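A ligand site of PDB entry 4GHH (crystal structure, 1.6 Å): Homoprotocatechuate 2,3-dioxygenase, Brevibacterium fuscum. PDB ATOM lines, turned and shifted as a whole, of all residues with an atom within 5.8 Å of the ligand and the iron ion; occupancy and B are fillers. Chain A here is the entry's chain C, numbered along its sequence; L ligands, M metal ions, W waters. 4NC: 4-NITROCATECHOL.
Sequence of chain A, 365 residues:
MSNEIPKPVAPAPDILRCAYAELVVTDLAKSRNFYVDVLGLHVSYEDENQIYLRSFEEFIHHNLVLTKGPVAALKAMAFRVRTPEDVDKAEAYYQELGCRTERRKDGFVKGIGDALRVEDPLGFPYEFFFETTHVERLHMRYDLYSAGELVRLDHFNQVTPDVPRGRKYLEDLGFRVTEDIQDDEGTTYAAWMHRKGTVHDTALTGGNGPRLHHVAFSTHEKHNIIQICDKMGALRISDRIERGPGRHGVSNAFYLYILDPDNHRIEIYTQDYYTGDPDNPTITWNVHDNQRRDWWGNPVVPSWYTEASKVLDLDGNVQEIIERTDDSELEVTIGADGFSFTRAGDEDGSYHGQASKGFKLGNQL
The backbone carbonyl oxygen (O) of Arg 292 lies close to an oxygen (O11) of the ligand, 3.2 Å away. Trp 192 touches the ligand (NE1 to C6, 3.3 Å). Arg 243 touches the ligand (NH2 to O10, 3.5 Å). Val 250 touches the ligand (O to C5, 3.1 Å). Ser 251 touches the ligand. Tyr 269 touches the ligand. Hydrophobic or aromatic side chains within 4 Å of the ligand: His 155, Trp 192, His 200, His 214, His 248, Val 250, Tyr 257 and Tyr 269. Of the 20 residues printed, 13 come within 4 Å of the ligand. The nearest printed residue that does not touch the ligand is Trp 304 (4.2 Å).
Water W1 lies within hydrogen-bond range of the side-chain amide nitrogen of Asn 157 (2.9 Å) and a ring nitrogen (NE2) of His 200 (3.0 Å).
OE1 of Glu 267 is bound to the iron ion. O7 of the ligand binds the iron ion (2.1 Å). The iron ion is bound by O8 of the ligand (2.2 Å). NE2 of His 214 is bound to the iron ion (2.2 Å). The iron ion is bound by NE2 of His 155 (2.2 Å). Water W1 binds the iron ion (2.4 Å). The iron ion has six donor atoms within binding distance.
The side-chain carboxylate of Glu 267 sits at hydrogen-bond distance from the side-chain hydroxyl of Tyr 257, 3.2 Å away. The backbone NH (N) of Asn 157 lies within hydrogen-bond range of the backbone carbonyl oxygen (O) of His 214 (3.1 Å). NE2 of His 200 lies close to ND1 of His 155, at 3.2 Å. A ring nitrogen (NE2) of His 248 lies close to the side-chain hydroxyl (OH) of Tyr 257, 3.3 Å away. The backbone carbonyl oxygen (O) of Arg 293 lies within hydrogen-bond range of a ring nitrogen (ND1) of His 248, 3.0 Å away. The backbone carbonyl oxygen (O) of Arg 293 lies within hydrogen-bond range of the guanidinium group (NH2) of Arg 243, at 3.3 Å. The backbone NH (N) of Val 250 sits at hydrogen-bond distance from the backbone carbonyl oxygen (O) of Arg 292, 2.8 Å away. O of Arg 292 lies close to N of Gly 249, at 3.3 Å.
O8 of the ligand sits close to OH of Tyr 257. A ring nitrogen (NE2) of His 200 sits close to an oxygen (O7) of the ligand (3.0 Å). The guanidinium group (NH1) of Arg 293 lies within hydrogen-bond range of an oxygen (O10) of the ligand (3.1 Å). An oxygen (O11) of the ligand lies within hydrogen-bond range of a ring nitrogen (ND1) of His 248, 3.3 Å away.
His 200 touches the iron ion (NE2 to FE, 3.8 Å). Four residues have an atom within 4 Å of the iron ion: His 155, His 200, His 214 and Glu 267.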
ATOM      1  N   HIS A 155      17.363  22.050   8.681  1.00  0.00           N
ATOM      2  CA  HIS A 155      16.173  22.787   9.137  1.00  0.00           C
ATOM      3  C   HIS A 155      15.347  22.010  10.115  1.00  0.00           C
ATOM      4  O   HIS A 155      15.543  20.806  10.269  1.00  0.00           O
ATOM      5  CB  HIS A 155      15.288  23.219   7.952  1.00  0.00           C
ATOM      6  CG  HIS A 155      14.705  22.087   7.149  1.00  0.00           C
ATOM      7  ND1 HIS A 155      15.296  21.580   6.013  1.00  0.00           N
ATOM      8  CD2 HIS A 155      13.509  21.405   7.299  1.00  0.00           C
ATOM      9  CE1 HIS A 155      14.503  20.621   5.496  1.00  0.00           C
ATOM     10  NE2 HIS A 155      13.423  20.495   6.287  1.00  0.00           N
ATOM     11  N   PHE A 156      14.367  22.704  10.698  1.00  0.00           N
ATOM     12  CA  PHE A 156      13.297  22.096  11.472  1.00  0.00           C
ATOM     13  C   PHE A 156      11.971  22.336  10.729  1.00  0.00           C
ATOM     14  O   PHE A 156      11.871  23.216   9.887  1.00  0.00           O
ATOM     15  CB  PHE A 156      13.169  22.756  12.852  1.00  0.00           C
ATOM     16  CG  PHE A 156      14.452  22.881  13.612  1.00  0.00           C
ATOM     17  CD1 PHE A 156      15.237  21.764  13.905  1.00  0.00           C
ATOM     18  CD2 PHE A 156      14.886  24.105  14.060  1.00  0.00           C
ATOM     19  CE1 PHE A 156      16.407  21.881  14.642  1.00  0.00           C
ATOM     20  CE2 PHE A 156      16.040  24.222  14.806  1.00  0.00           C
ATOM     21  CZ  PHE A 156      16.811  23.132  15.076  1.00  0.00           C
ATOM     22  N   ASN A 157      10.967  21.555  11.053  1.00  0.00           N
ATOM     23  CA  ASN A 157       9.602  21.761  10.560  1.00  0.00           C
ATOM     24  C   ASN A 157       8.651  21.547  11.728  1.00  0.00           C
ATOM     25  O   ASN A 157       8.705  20.532  12.420  1.00  0.00           O
ATOM     26  CB  ASN A 157       9.286  20.881   9.341  1.00  0.00           C
ATOM     27  CG  ASN A 157       7.914  21.140   8.749  1.00  0.00           C
ATOM     28  OD1 ASN A 157       6.865  21.041   9.434  1.00  0.00           O
ATOM     29  ND2 ASN A 157       7.911  21.468   7.455  1.00  0.00           N
ATOM     30  N   ILE A 181       2.300  27.356   0.509  1.00  0.00           N
ATOM     31  CA  ILE A 181       1.196  26.628  -0.132  1.00  0.00           C
ATOM     32  C   ILE A 181      -0.101  27.288   0.356  1.00  0.00           C
ATOM     33  O   ILE A 181      -0.343  27.411   1.564  1.00  0.00           O
ATOM     34  CB  ILE A 181       1.177  25.109   0.196  1.00  0.00           C
ATOM     35  CG1 ILE A 181       2.461  24.434  -0.303  1.00  0.00           C
ATOM     36  CG2 ILE A 181      -0.055  24.422  -0.399  1.00  0.00           C
ATOM     37  CD1 ILE A 181       2.599  22.982   0.169  1.00  0.00           C
ATOM     38  N   TRP A 192       7.636  28.215   4.413  1.00  0.00           N
ATOM     39  CA  TRP A 192       9.058  27.939   4.603  1.00  0.00           C
ATOM     40  C   TRP A 192       9.784  29.240   4.786  1.00  0.00           C
ATOM     41  O   TRP A 192       9.526  30.180   4.076  1.00  0.00           O
ATOM     42  CB  TRP A 192       9.615  27.219   3.369  1.00  0.00           C
ATOM     43  CG  TRP A 192       9.183  25.788   3.281  1.00  0.00           C
ATOM     44  CD1 TRP A 192       9.958  24.666   3.546  1.00  0.00           C
ATOM     45  CD2 TRP A 192       7.873  25.267   2.854  1.00  0.00           C
ATOM     46  NE1 TRP A 192       9.228  23.508   3.370  1.00  0.00           N
ATOM     47  CE2 TRP A 192       7.973  23.800   2.942  1.00  0.00           C
ATOM     48  CE3 TRP A 192       6.657  25.831   2.453  1.00  0.00           C
ATOM     49  CZ2 TRP A 192       6.896  22.967   2.605  1.00  0.00           C
ATOM     50  CZ3 TRP A 192       5.610  24.976   2.121  1.00  0.00           C
ATOM     51  CH2 TRP A 192       5.725  23.576   2.190  1.00  0.00           C
ATOM     52  N   HIS A 200      15.112  27.154   3.849  1.00  0.00           N
ATOM     53  CA  HIS A 200      14.603  27.322   5.219  1.00  0.00           C
ATOM     54  C   HIS A 200      15.549  26.940   6.314  1.00  0.00           C
ATOM     55  O   HIS A 200      16.415  26.074   6.112  1.00  0.00           O
ATOM     56  CB  HIS A 200      13.244  26.616   5.430  1.00  0.00           C
ATOM     57  CG  HIS A 200      13.201  25.154   5.060  1.00  0.00           C
ATOM     58  ND1 HIS A 200      13.924  24.634   4.043  1.00  0.00           N
ATOM     59  CD2 HIS A 200      12.415  24.104   5.553  1.00  0.00           C
ATOM     60  CE1 HIS A 200      13.600  23.332   3.894  1.00  0.00           C
ATOM     61  NE2 HIS A 200      12.666  23.015   4.780  1.00  0.00           N
ATOM     62  N   HIS A 214       9.489  17.396  11.830  1.00  0.00           N
ATOM     63  CA  HIS A 214      10.759  16.695  11.569  1.00  0.00           C
ATOM     64  C   HIS A 214      11.956  17.552  11.813  1.00  0.00           C
ATOM     65  O   HIS A 214      11.863  18.767  11.912  1.00  0.00           O
ATOM     66  CB  HIS A 214      10.806  16.081  10.143  1.00  0.00           C
ATOM     67  CG  HIS A 214      10.660  17.074   9.009  1.00  0.00           C
ATOM     68  ND1 HIS A 214       9.461  17.378   8.460  1.00  0.00           N
ATOM     69  CD2 HIS A 214      11.598  17.755   8.287  1.00  0.00           C
ATOM     70  CE1 HIS A 214       9.641  18.250   7.444  1.00  0.00           C
ATOM     71  NE2 HIS A 214      10.930  18.475   7.329  1.00  0.00           N
ATOM     72  N   ALA A 216      15.741  17.968   9.797  1.00  0.00           N
ATOM     73  CA  ALA A 216      16.324  17.617   8.491  1.00  0.00           C
ATOM     74  C   ALA A 216      17.816  17.778   8.456  1.00  0.00           C
ATOM     75  O   ALA A 216      18.320  18.835   8.872  1.00  0.00           O
ATOM     76  CB  ALA A 216      15.722  18.470   7.375  1.00  0.00           C
ATOM     77  N   ARG A 243       8.250   7.979   3.689  1.00  0.00           N
ATOM     78  CA  ARG A 243       7.889   8.641   2.455  1.00  0.00           C
ATOM     79  C   ARG A 243       9.148   8.990   1.678  1.00  0.00           C
ATOM     80  O   ARG A 243      10.104   9.478   2.244  1.00  0.00           O
ATOM     81  CB  ARG A 243       7.104   9.926   2.771  1.00  0.00           C
ATOM     82  CG  ARG A 243       6.879  10.862   1.605  1.00  0.00           C
ATOM     83  CD  ARG A 243       5.930  12.035   1.900  1.00  0.00           C
ATOM     84  NE  ARG A 243       6.074  12.956   0.778  1.00  0.00           N
ATOM     85  CZ  ARG A 243       6.206  14.290   0.854  1.00  0.00           C
ATOM     86  NH1 ARG A 243       6.024  14.954   1.984  1.00  0.00           N
ATOM     87  NH2 ARG A 243       6.486  14.973  -0.246  1.00  0.00           N
ATOM     88  N   HIS A 248      11.162  17.248  -4.094  1.00  0.00           N
ATOM     89  CA  HIS A 248      10.139  18.171  -3.670  1.00  0.00           C
ATOM     90  C   HIS A 248       9.796  19.154  -4.763  1.00  0.00           C
ATOM     91  O   HIS A 248      10.640  19.533  -5.573  1.00  0.00           O
ATOM     92  CB  HIS A 248      10.609  18.999  -2.465  1.00  0.00           C
ATOM     93  CG  HIS A 248      10.614  18.275  -1.142  1.00  0.00           C
ATOM     94  ND1 HIS A 248       9.524  17.632  -0.655  1.00  0.00           N
ATOM     95  CD2 HIS A 248      11.591  18.234  -0.133  1.00  0.00           C
ATOM     96  CE1 HIS A 248       9.815  17.140   0.578  1.00  0.00           C
ATOM     97  NE2 HIS A 248      11.067  17.515   0.894  1.00  0.00           N
ATOM     98  N   GLY A 249       8.543  19.600  -4.774  1.00  0.00           N
ATOM     99  CA  GLY A 249       8.162  20.775  -5.563  1.00  0.00           C
ATOM    100  C   GLY A 249       8.680  22.025  -4.833  1.00  0.00           C
ATOM    101  O   GLY A 249       9.682  22.623  -5.222  1.00  0.00           O
ATOM    102  N   VAL A 250       7.995  22.386  -3.746  1.00  0.00           N
ATOM    103  CA  VAL A 250       8.528  23.362  -2.794  1.00  0.00           C
ATOM    104  C   VAL A 250       9.976  22.979  -2.382  1.00  0.00           C
ATOM    105  O   VAL A 250      10.207  21.874  -1.927  1.00  0.00           O
ATOM    106  CB  VAL A 250       7.685  23.401  -1.494  1.00  0.00           C
ATOM    107  CG1 VAL A 250       8.366  24.330  -0.462  1.00  0.00           C
ATOM    108  CG2 VAL A 250       6.244  23.803  -1.826  1.00  0.00           C
ATOM    109  N   SER A 251      10.899  23.897  -2.589  1.00  0.00           N
ATOM    110  CA  SER A 251      12.343  23.795  -2.257  1.00  0.00           C
ATOM    111  C   SER A 251      13.182  23.180  -3.351  1.00  0.00           C
ATOM    112  O   SER A 251      14.383  23.408  -3.364  1.00  0.00           O
ATOM    113  CB  SER A 251      12.655  23.074  -0.925  1.00  0.00           C
ATOM    114  OG  SER A 251      12.629  21.655  -1.062  1.00  0.00           O
ATOM    115  N   TYR A 257      12.019  10.759   4.014  1.00  0.00           N
ATOM    116  CA  TYR A 257      11.590  10.788   5.414  1.00  0.00           C
ATOM    117  C   TYR A 257      11.632   9.404   6.055  1.00  0.00           C
ATOM    118  O   TYR A 257      11.067   8.458   5.504  1.00  0.00           O
ATOM    119  CB  TYR A 257      10.194  11.336   5.571  1.00  0.00           C
ATOM    120  CG  TYR A 257      10.015  12.735   5.053  1.00  0.00           C
ATOM    121  CD1 TYR A 257      10.261  13.857   5.850  1.00  0.00           C
ATOM    122  CD2 TYR A 257       9.595  12.952   3.764  1.00  0.00           C
ATOM    123  CE1 TYR A 257      10.055  15.151   5.363  1.00  0.00           C
ATOM    124  CE2 TYR A 257       9.389  14.222   3.276  1.00  0.00           C
ATOM    125  CZ  TYR A 257       9.635  15.325   4.062  1.00  0.00           C
ATOM    126  OH  TYR A 257       9.422  16.552   3.549  1.00  0.00           O
ATOM    127  N   GLU A 267      14.143  13.988   8.190  1.00  0.00           N
ATOM    128  CA  GLU A 267      14.258  14.181   6.740  1.00  0.00           C
ATOM    129  C   GLU A 267      15.737  14.175   6.361  1.00  0.00           C
ATOM    130  O   GLU A 267      16.555  14.740   7.048  1.00  0.00           O
ATOM    131  CB  GLU A 267      13.621  15.477   6.294  1.00  0.00           C
ATOM    132  CG  GLU A 267      13.520  15.607   4.784  1.00  0.00           C
ATOM    133  CD  GLU A 267      12.909  16.911   4.324  1.00  0.00           C
ATOM    134  OE1 GLU A 267      12.775  17.791   5.166  1.00  0.00           O
ATOM    135  OE2 GLU A 267      12.579  17.041   3.130  1.00  0.00           O
ATOM    136  N   TYR A 269      17.922  15.430   2.969  1.00  0.00           N
ATOM    137  CA  TYR A 269      17.579  16.520   2.083  1.00  0.00           C
ATOM    138  C   TYR A 269      18.846  16.981   1.344  1.00  0.00           C
ATOM    139  O   TYR A 269      19.925  16.987   1.902  1.00  0.00           O
ATOM    140  CB  TYR A 269      17.065  17.644   2.991  1.00  0.00           C
ATOM    141  CG  TYR A 269      16.609  18.971   2.432  1.00  0.00           C
ATOM    142  CD1 TYR A 269      15.261  19.224   2.197  1.00  0.00           C
ATOM    143  CD2 TYR A 269      17.506  20.034   2.229  1.00  0.00           C
ATOM    144  CE1 TYR A 269      14.806  20.460   1.762  1.00  0.00           C
ATOM    145  CE2 TYR A 269      17.056  21.265   1.758  1.00  0.00           C
ATOM    146  CZ  TYR A 269      15.699  21.489   1.575  1.00  0.00           C
ATOM    147  OH  TYR A 269      15.250  22.744   1.162  1.00  0.00           O
ATOM    148  N   ARG A 292       3.401  19.782  -5.980  1.00  0.00           N
ATOM    149  CA  ARG A 292       3.914  20.721  -4.971  1.00  0.00           C
ATOM    150  C   ARG A 292       4.809  20.077  -3.910  1.00  0.00           C
ATOM    151  O   ARG A 292       5.737  20.705  -3.446  1.00  0.00           O
ATOM    152  CB  ARG A 292       2.756  21.506  -4.324  1.00  0.00           C
ATOM    153  CG  ARG A 292       1.995  20.746  -3.268  1.00  0.00           C
ATOM    154  CD  ARG A 292       0.625  21.258  -2.907  1.00  0.00           C
ATOM    155  NE  ARG A 292       0.096  20.365  -1.860  1.00  0.00           N
ATOM    156  CZ  ARG A 292      -0.412  19.159  -2.081  1.00  0.00           C
ATOM    157  NH1 ARG A 292      -0.503  18.686  -3.305  1.00  0.00           N
ATOM    158  NH2 ARG A 292      -0.795  18.391  -1.067  1.00  0.00           N
ATOM    159  N   ARG A 293       4.471  18.852  -3.492  1.00  0.00           N
ATOM    160  CA  ARG A 293       5.152  18.192  -2.397  1.00  0.00           C
ATOM    161  C   ARG A 293       6.102  17.139  -2.938  1.00  0.00           C
ATOM    162  O   ARG A 293       7.267  17.116  -2.565  1.00  0.00           O
ATOM    163  CB  ARG A 293       4.143  17.626  -1.383  1.00  0.00           C
ATOM    164  CG  ARG A 293       3.586  18.756  -0.491  1.00  0.00           C
ATOM    165  CD  ARG A 293       3.079  18.259   0.843  1.00  0.00           C
ATOM    166  NE  ARG A 293       2.539  19.330   1.694  1.00  0.00           N
ATOM    167  CZ  ARG A 293       3.250  20.058   2.543  1.00  0.00           C
ATOM    168  NH1 ARG A 293       4.564  19.906   2.643  1.00  0.00           N
ATOM    169  NH2 ARG A 293       2.653  20.958   3.281  1.00  0.00           N
ATOM    170  N   ASP A 294       5.621  16.293  -3.833  1.00  0.00           N
ATOM    171  CA  ASP A 294       6.462  15.412  -4.599  1.00  0.00           C
ATOM    172  C   ASP A 294       6.293  15.827  -6.059  1.00  0.00           C
ATOM    173  O   ASP A 294       5.195  15.721  -6.640  1.00  0.00           O
ATOM    174  CB  ASP A 294       6.082  13.956  -4.416  1.00  0.00           C
ATOM    175  CG  ASP A 294       7.101  13.043  -5.042  1.00  0.00           C
ATOM    176  OD1 ASP A 294       8.147  12.747  -4.376  1.00  0.00           O
ATOM    177  OD2 ASP A 294       6.892  12.640  -6.215  1.00  0.00           O
ATOM    178  N   TRP A 304       2.072  11.158   7.137  1.00  0.00           N
ATOM    179  CA  TRP A 304       2.932  12.354   6.977  1.00  0.00           C
ATOM    180  C   TRP A 304       2.215  13.616   7.407  1.00  0.00           C
ATOM    181  O   TRP A 304       2.805  14.503   8.044  1.00  0.00           O
ATOM    182  CB  TRP A 304       3.415  12.445   5.547  1.00  0.00           C
ATOM    183  CG  TRP A 304       4.600  13.363   5.408  1.00  0.00           C
ATOM    184  CD1 TRP A 304       5.940  13.043   5.560  1.00  0.00           C
ATOM    185  CD2 TRP A 304       4.565  14.828   5.215  1.00  0.00           C
ATOM    186  NE1 TRP A 304       6.721  14.157   5.422  1.00  0.00           N
ATOM    187  CE2 TRP A 304       5.962  15.263   5.220  1.00  0.00           C
ATOM    188  CE3 TRP A 304       3.567  15.773   5.057  1.00  0.00           C
ATOM    189  CZ2 TRP A 304       6.314  16.591   5.066  1.00  0.00           C
ATOM    190  CZ3 TRP A 304       3.928  17.105   4.907  1.00  0.00           C
ATOM    191  CH2 TRP A 304       5.294  17.512   4.903  1.00  0.00           C
HETATM  192  C1  4NC L   1      10.833  20.326   2.909  1.00  0.00           C
HETATM  193  C2  4NC L   1       9.677  19.486   3.417  1.00  0.00           C
HETATM  194  C3  4NC L   1       8.457  19.418   2.698  1.00  0.00           C
HETATM  195  C4  4NC L   1       8.384  20.032   1.396  1.00  0.00           C
HETATM  196  C5  4NC L   1       9.449  20.866   0.949  1.00  0.00           C
HETATM  197  C6  4NC L   1      10.636  21.056   1.683  1.00  0.00           C
HETATM  198  O7  4NC L   1      12.014  20.302   3.618  1.00  0.00           O
HETATM  199  O8  4NC L   1       9.846  18.787   4.563  1.00  0.00           O
HETATM  200  N9  4NC L   1       7.289  19.646   0.607  1.00  0.00           N
HETATM  201  O10 4NC L   1       6.630  18.310   0.934  1.00  0.00           O
HETATM  202  O11 4NC L   1       7.337  20.041  -0.711  1.00  0.00           O
HETATM  203 FE    FE M   1      11.654  19.451   5.533  1.00  0.00          FE
HETATM  204  O   HOH W   1      10.422  21.492   5.983  1.00  0.00           O
